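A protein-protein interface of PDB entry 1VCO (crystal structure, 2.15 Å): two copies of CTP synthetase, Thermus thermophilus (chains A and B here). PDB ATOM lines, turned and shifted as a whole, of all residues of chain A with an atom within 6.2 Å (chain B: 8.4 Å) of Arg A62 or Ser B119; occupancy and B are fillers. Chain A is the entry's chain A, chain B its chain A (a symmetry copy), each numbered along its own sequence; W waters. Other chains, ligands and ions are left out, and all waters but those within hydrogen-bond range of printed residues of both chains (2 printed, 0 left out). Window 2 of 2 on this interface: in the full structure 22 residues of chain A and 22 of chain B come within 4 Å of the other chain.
N of Val B122 sits close to ND2 of Asn A55 (2.7 Å).
The side-chain carboxylate (OE1) of Glu B112 sits at hydrogen-bond distance from the side-chain hydroxyl (OG1) of Thr A60 (2.9 Å).
The backbone carbonyl oxygen (O) of Thr A60 lies close to the side-chain hydroxyl (OG) of Ser B119 (3.3 Å).
The side-chain amide oxygen (OD1) of Asn A55 sits close to the backbone carbonyl oxygen (O) of Gln B120, at 3.5 Å.
OE1 of Glu B112 sits close to OD1 of Asn A55 (3.1 Å).
The backbone carbonyl oxygen (O) of Tyr B117 lies close to the side-chain amide oxygen (OE1) of Gln B120 (2.9 Å).
Thr B121 touches Asn A55 (CA to ND2, 3.5 Å).
Ser B119 touches Met A61 (O to CA, 3.5 Å).
N of Arg A62 touches O of Ser B119, 3.9 Å away.
Of the printed residues of chain B, Arg A62 touches Ser B119 (3.9 Å).
Ser B119 touches just these residues of chain A: Thr A60 (3.1 Å), Met A61 (3.5 Å) and Arg A62 (3.9 Å).
Of the printed residues of chain A, Glu B112 touches Asn A55 (3.1 Å) and Thr A60 (2.9 Å).
Of the printed residues of chain A, Gln B120 touches Asn A55.
Printed residues of chain A within 4 Å of Val B122: Asn A55.
Glu B116 touches none of the printed residues of chain A.
Val A69 touches none of the printed residues of chain B.
The nearest residue of chain B that does not touch Arg A62 is Gln B120 (6.0 Å).
The nearest residue of chain A that does not touch Ser B119 is His A66 (4.9 Å).
Of the 12 printed residues of chain A, 4 touch a printed residue of chain B.
No position is printed for both chains.
Water W2 lies within hydrogen-bond range of the side-chain hydroxyl of Thr B121 and the side-chain sulfur of Met A61.
Water W1 lies within hydrogen-bond range of the backbone carbonyl oxygen of Gln B120, the backbone NH of Ser B119 and the side-chain hydroxyl of Thr A60.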
ATOM      1  N   ASN A  55      -7.151  -7.241 -23.685  1.00  0.00           N
ATOM      2  CA  ASN A  55      -7.568  -6.125 -24.536  1.00  0.00           C
ATOM      3  C   ASN A  55      -8.136  -6.716 -25.827  1.00  0.00           C
ATOM      4  O   ASN A  55      -7.528  -7.605 -26.429  1.00  0.00           O
ATOM      5  CB  ASN A  55      -6.374  -5.229 -24.891  1.00  0.00           C
ATOM      6  CG  ASN A  55      -5.721  -4.606 -23.673  1.00  0.00           C
ATOM      7  OD1 ASN A  55      -5.952  -3.436 -23.356  1.00  0.00           O
ATOM      8  ND2 ASN A  55      -4.898  -5.386 -22.981  1.00  0.00           N
ATOM      9  N   ALA A  58      -5.466  -3.419 -29.812  1.00  0.00           N
ATOM     10  CA  ALA A  58      -4.522  -2.432 -29.297  1.00  0.00           C
ATOM     11  C   ALA A  58      -5.068  -1.012 -29.354  1.00  0.00           C
ATOM     12  O   ALA A  58      -4.343  -0.062 -29.093  1.00  0.00           O
ATOM     13  CB  ALA A  58      -3.202  -2.513 -30.074  1.00  0.00           C
ATOM     14  N   THR A  60      -7.128   0.735 -27.346  1.00  0.00           N
ATOM     15  CA  THR A  60      -7.229   1.545 -26.132  1.00  0.00           C
ATOM     16  C   THR A  60      -5.874   1.845 -25.499  1.00  0.00           C
ATOM     17  O   THR A  60      -5.799   2.542 -24.488  1.00  0.00           O
ATOM     18  CB  THR A  60      -8.114   0.861 -25.070  1.00  0.00           C
ATOM     19  OG1 THR A  60      -7.506  -0.370 -24.649  1.00  0.00           O
ATOM     20  CG2 THR A  60      -9.495   0.572 -25.646  1.00  0.00           C
ATOM     21  N   MET A  61      -4.808   1.325 -26.097  1.00  0.00           N
ATOM     22  CA  MET A  61      -3.459   1.538 -25.578  1.00  0.00           C
ATOM     23  C   MET A  61      -2.858   2.837 -26.111  1.00  0.00           C
ATOM     24  O   MET A  61      -3.435   3.480 -26.984  1.00  0.00           O
ATOM     25  CB  MET A  61      -2.565   0.361 -25.973  1.00  0.00           C
ATOM     26  CG  MET A  61      -3.003  -0.967 -25.378  1.00  0.00           C
ATOM     27  SD  MET A  61      -2.031  -2.340 -26.009  1.00  0.00           S
ATOM     28  CE  MET A  61      -3.164  -3.712 -25.784  1.00  0.00           C
ATOM     29  N   ARG A  62      -1.711   3.230 -25.564  1.00  0.00           N
ATOM     30  CA  ARG A  62      -1.029   4.440 -26.019  1.00  0.00           C
ATOM     31  C   ARG A  62      -0.452   4.055 -27.375  1.00  0.00           C
ATOM     32  O   ARG A  62       0.166   3.002 -27.511  1.00  0.00           O
ATOM     33  CB  ARG A  62       0.089   4.823 -25.050  1.00  0.00           C
ATOM     34  N   PRO A  63      -0.668   4.890 -28.400  1.00  0.00           N
ATOM     35  CA  PRO A  63      -0.170   4.628 -29.755  1.00  0.00           C
ATOM     36  C   PRO A  63       1.348   4.541 -29.918  1.00  0.00           C
ATOM     37  O   PRO A  63       1.829   3.810 -30.783  1.00  0.00           O
ATOM     38  CB  PRO A  63      -0.760   5.781 -30.568  1.00  0.00           C
ATOM     39  CG  PRO A  63      -1.995   6.151 -29.805  1.00  0.00           C
ATOM     40  CD  PRO A  63      -1.526   6.085 -28.380  1.00  0.00           C
ATOM     41  N   TYR A  64       2.098   5.269 -29.090  1.00  0.00           N
ATOM     42  CA  TYR A  64       3.563   5.269 -29.201  1.00  0.00           C
ATOM     43  C   TYR A  64       4.350   4.914 -27.937  1.00  0.00           C
ATOM     44  O   TYR A  64       5.170   3.998 -27.941  1.00  0.00           O
ATOM     45  CB  TYR A  64       4.060   6.641 -29.679  1.00  0.00           C
ATOM     46  CG  TYR A  64       3.424   7.143 -30.955  1.00  0.00           C
ATOM     47  CD1 TYR A  64       2.208   7.827 -30.936  1.00  0.00           C
ATOM     48  CD2 TYR A  64       4.040   6.927 -32.184  1.00  0.00           C
ATOM     49  CE1 TYR A  64       1.621   8.283 -32.121  1.00  0.00           C
ATOM     50  CE2 TYR A  64       3.469   7.372 -33.365  1.00  0.00           C
ATOM     51  CZ  TYR A  64       2.263   8.048 -33.333  1.00  0.00           C
ATOM     52  OH  TYR A  64       1.715   8.474 -34.519  1.00  0.00           O
ATOM     53  N   GLU A  65       4.098   5.673 -26.875  1.00  0.00           N
ATOM     54  CA  GLU A  65       4.773   5.546 -25.590  1.00  0.00           C
ATOM     55  C   GLU A  65       5.306   4.179 -25.151  1.00  0.00           C
ATOM     56  O   GLU A  65       6.506   4.035 -24.897  1.00  0.00           O
ATOM     57  CB  GLU A  65       3.881   6.122 -24.487  1.00  0.00           C
ATOM     58  CG  GLU A  65       4.563   6.184 -23.133  1.00  0.00           C
ATOM     59  CD  GLU A  65       3.794   7.010 -22.123  1.00  0.00           C
ATOM     60  OE1 GLU A  65       4.232   7.075 -20.957  1.00  0.00           O
ATOM     61  OE2 GLU A  65       2.755   7.596 -22.494  1.00  0.00           O
ATOM     62  N   HIS A  66       4.435   3.183 -25.046  1.00  0.00           N
ATOM     63  CA  HIS A  66       4.877   1.858 -24.613  1.00  0.00           C
ATOM     64  C   HIS A  66       5.118   0.925 -25.798  1.00  0.00           C
ATOM     65  O   HIS A  66       4.910  -0.283 -25.700  1.00  0.00           O
ATOM     66  CB  HIS A  66       3.831   1.251 -23.675  1.00  0.00           C
ATOM     67  CG  HIS A  66       3.442   2.157 -22.548  1.00  0.00           C
ATOM     68  ND1 HIS A  66       4.314   2.506 -21.540  1.00  0.00           N
ATOM     69  CD2 HIS A  66       2.287   2.817 -22.293  1.00  0.00           C
ATOM     70  CE1 HIS A  66       3.714   3.344 -20.713  1.00  0.00           C
ATOM     71  NE2 HIS A  66       2.484   3.550 -21.147  1.00  0.00           N
ATOM     72  N   GLY A  67       5.570   1.493 -26.910  1.00  0.00           N
ATOM     73  CA  GLY A  67       5.807   0.698 -28.100  1.00  0.00           C
ATOM     74  C   GLY A  67       4.721   0.995 -29.119  1.00  0.00           C
ATOM     75  O   GLY A  67       3.556   1.165 -28.762  1.00  0.00           O
ATOM     76  N   GLU A  68       5.104   1.065 -30.387  1.00  0.00           N
ATOM     77  CA  GLU A  68       4.173   1.360 -31.465  1.00  0.00           C
ATOM     78  C   GLU A  68       3.002   0.394 -31.610  1.00  0.00           C
ATOM     79  O   GLU A  68       3.123  -0.806 -31.347  1.00  0.00           O
ATOM     80  CB  GLU A  68       4.929   1.417 -32.797  1.00  0.00           C
ATOM     81  CG  GLU A  68       4.221   0.711 -33.946  1.00  0.00           C
ATOM     82  CD  GLU A  68       5.060   0.651 -35.207  1.00  0.00           C
ATOM     83  OE1 GLU A  68       4.906  -0.311 -35.985  1.00  0.00           O
ATOM     84  OE2 GLU A  68       5.867   1.568 -35.426  1.00  0.00           O
ATOM     85  N   VAL A  69       1.868   0.946 -32.025  1.00  0.00           N
ATOM     86  CA  VAL A  69       0.671   0.169 -32.291  1.00  0.00           C
ATOM     87  C   VAL A  69       0.558   0.227 -33.811  1.00  0.00           C
ATOM     88  O   VAL A  69       0.415   1.307 -34.393  1.00  0.00           O
ATOM     89  CB  VAL A  69      -0.596   0.794 -31.660  1.00  0.00           C
ATOM     90  CG1 VAL A  69      -1.836   0.063 -32.158  1.00  0.00           C
ATOM     91  CG2 VAL A  69      -0.528   0.705 -30.136  1.00  0.00           C
ATOM     92  N   LYS B 111     -14.916  -3.076 -19.404  1.00  0.00           N
ATOM     93  CA  LYS B 111     -14.186  -1.996 -18.756  1.00  0.00           C
ATOM     94  C   LYS B 111     -13.021  -1.484 -19.594  1.00  0.00           C
ATOM     95  O   LYS B 111     -12.781  -0.276 -19.634  1.00  0.00           O
ATOM     96  CB  LYS B 111     -13.689  -2.439 -17.383  1.00  0.00           C
ATOM     97  N   GLU B 112     -12.290  -2.372 -20.269  1.00  0.00           N
ATOM     98  CA  GLU B 112     -11.171  -1.881 -21.062  1.00  0.00           C
ATOM     99  C   GLU B 112     -11.612  -1.286 -22.389  1.00  0.00           C
ATOM    100  O   GLU B 112     -10.879  -0.495 -22.968  1.00  0.00           O
ATOM    101  CB  GLU B 112     -10.102  -2.962 -21.281  1.00  0.00           C
ATOM    102  CG  GLU B 112     -10.359  -3.982 -22.354  1.00  0.00           C
ATOM    103  CD  GLU B 112      -9.930  -3.538 -23.754  1.00  0.00           C
ATOM    104  OE1 GLU B 112      -8.909  -2.836 -23.928  1.00  0.00           O
ATOM    105  OE2 GLU B 112     -10.619  -3.932 -24.700  1.00  0.00           O
ATOM    106  N   ARG B 114     -14.119   0.626 -22.610  1.00  0.00           N
ATOM    107  CA  ARG B 114     -14.515   1.973 -22.203  1.00  0.00           C
ATOM    108  C   ARG B 114     -13.269   2.772 -21.845  1.00  0.00           C
ATOM    109  O   ARG B 114     -13.356   3.946 -21.492  1.00  0.00           O
ATOM    110  CB  ARG B 114     -15.466   1.929 -21.002  1.00  0.00           C
ATOM    111  CG  ARG B 114     -16.836   1.340 -21.318  1.00  0.00           C
ATOM    112  CD  ARG B 114     -17.856   1.692 -20.248  1.00  0.00           C
ATOM    113  NE  ARG B 114     -17.543   1.112 -18.947  1.00  0.00           N
ATOM    114  CZ  ARG B 114     -17.857  -0.129 -18.585  1.00  0.00           C
ATOM    115  NH1 ARG B 114     -18.499  -0.927 -19.427  1.00  0.00           N
ATOM    116  NH2 ARG B 114     -17.527  -0.572 -17.377  1.00  0.00           N
ATOM    117  N   GLY B 115     -12.112   2.123 -21.943  1.00  0.00           N
ATOM    118  CA  GLY B 115     -10.856   2.787 -21.645  1.00  0.00           C
ATOM    119  C   GLY B 115     -10.607   3.051 -20.174  1.00  0.00           C
ATOM    120  O   GLY B 115      -9.694   3.792 -19.816  1.00  0.00           O
ATOM    121  N   GLU B 116     -11.406   2.434 -19.315  1.00  0.00           N
ATOM    122  CA  GLU B 116     -11.264   2.625 -17.880  1.00  0.00           C
ATOM    123  C   GLU B 116     -10.002   2.032 -17.258  1.00  0.00           C
ATOM    124  O   GLU B 116      -9.751   2.225 -16.068  1.00  0.00           O
ATOM    125  CB  GLU B 116     -12.506   2.098 -17.169  1.00  0.00           C
ATOM    126  CG  GLU B 116     -13.605   3.145 -17.080  1.00  0.00           C
ATOM    127  CD  GLU B 116     -14.992   2.552 -17.104  1.00  0.00           C
ATOM    128  OE1 GLU B 116     -15.207   1.516 -16.435  1.00  0.00           O
ATOM    129  OE2 GLU B 116     -15.865   3.134 -17.791  1.00  0.00           O
ATOM    130  N   TYR B 117      -9.210   1.308 -18.045  1.00  0.00           N
ATOM    131  CA  TYR B 117      -7.967   0.761 -17.516  1.00  0.00           C
ATOM    132  C   TYR B 117      -6.816   1.707 -17.827  1.00  0.00           C
ATOM    133  O   TYR B 117      -5.649   1.391 -17.616  1.00  0.00           O
ATOM    134  CB  TYR B 117      -7.698  -0.646 -18.059  1.00  0.00           C
ATOM    135  CG  TYR B 117      -8.459  -1.700 -17.287  1.00  0.00           C
ATOM    136  CD1 TYR B 117      -9.533  -2.381 -17.860  1.00  0.00           C
ATOM    137  CD2 TYR B 117      -8.144  -1.972 -15.954  1.00  0.00           C
ATOM    138  CE1 TYR B 117     -10.276  -3.303 -17.121  1.00  0.00           C
ATOM    139  CE2 TYR B 117      -8.882  -2.890 -15.208  1.00  0.00           C
ATOM    140  CZ  TYR B 117      -9.944  -3.549 -15.796  1.00  0.00           C
ATOM    141  OH  TYR B 117     -10.679  -4.446 -15.059  1.00  0.00           O
ATOM    142  N   LEU B 118      -7.170   2.881 -18.341  1.00  0.00           N
ATOM    143  CA  LEU B 118      -6.203   3.931 -18.645  1.00  0.00           C
ATOM    144  C   LEU B 118      -5.043   3.590 -19.579  1.00  0.00           C
ATOM    145  O   LEU B 118      -3.887   3.853 -19.256  1.00  0.00           O
ATOM    146  CB  LEU B 118      -5.645   4.492 -17.331  1.00  0.00           C
ATOM    147  CG  LEU B 118      -6.595   5.328 -16.464  1.00  0.00           C
ATOM    148  CD1 LEU B 118      -7.912   4.603 -16.252  1.00  0.00           C
ATOM    149  CD2 LEU B 118      -5.924   5.622 -15.130  1.00  0.00           C
ATOM    150  N   SER B 119      -5.356   3.005 -20.731  1.00  0.00           N
ATOM    151  CA  SER B 119      -4.347   2.679 -21.738  1.00  0.00           C
ATOM    152  C   SER B 119      -3.338   1.576 -21.444  1.00  0.00           C
ATOM    153  O   SER B 119      -2.432   1.349 -22.249  1.00  0.00           O
ATOM    154  CB  SER B 119      -3.578   3.952 -22.123  1.00  0.00           C
ATOM    155  OG  SER B 119      -4.459   4.935 -22.644  1.00  0.00           O
ATOM    156  N   GLN B 120      -3.471   0.886 -20.319  1.00  0.00           N
ATOM    157  CA  GLN B 120      -2.521  -0.183 -20.017  1.00  0.00           C
ATOM    158  C   GLN B 120      -2.972  -1.525 -20.600  1.00  0.00           C
ATOM    159  O   GLN B 120      -4.132  -1.694 -20.983  1.00  0.00           O
ATOM    160  CB  GLN B 120      -2.323  -0.311 -18.503  1.00  0.00           C
ATOM    161  CG  GLN B 120      -3.483  -0.930 -17.763  1.00  0.00           C
ATOM    162  CD  GLN B 120      -3.425  -0.648 -16.276  1.00  0.00           C
ATOM    163  OE1 GLN B 120      -3.545   0.497 -15.856  1.00  0.00           O
ATOM    164  NE2 GLN B 120      -3.236  -1.692 -15.472  1.00  0.00           N
ATOM    165  N   THR B 121      -2.032  -2.463 -20.695  1.00  0.00           N
ATOM    166  CA  THR B 121      -2.319  -3.798 -21.203  1.00  0.00           C
ATOM    167  C   THR B 121      -3.038  -4.556 -20.102  1.00  0.00           C
ATOM    168  O   THR B 121      -2.519  -4.702 -18.999  1.00  0.00           O
ATOM    169  CB  THR B 121      -1.030  -4.555 -21.558  1.00  0.00           C
ATOM    170  OG1 THR B 121      -0.326  -3.835 -22.573  1.00  0.00           O
ATOM    171  CG2 THR B 121      -1.351  -5.943 -22.066  1.00  0.00           C
ATOM    172  N   VAL B 122      -4.232  -5.039 -20.410  1.00  0.00           N
ATOM    173  CA  VAL B 122      -5.038  -5.769 -19.443  1.00  0.00           C
ATOM    174  C   VAL B 122      -4.781  -7.274 -19.538  1.00  0.00           C
ATOM    175  O   VAL B 122      -4.773  -7.836 -20.625  1.00  0.00           O
ATOM    176  CB  VAL B 122      -6.531  -5.470 -19.681  1.00  0.00           C
ATOM    177  CG1 VAL B 122      -7.380  -6.180 -18.652  1.00  0.00           C
ATOM    178  CG2 VAL B 122      -6.758  -3.958 -19.624  1.00  0.00           C
HETATM  179  O   HOH W   1      -6.431  -0.053 -21.407  1.00  0.00           O
HETATM  180  O   HOH W   2       0.292  -1.402 -23.363  1.00  0.00           O
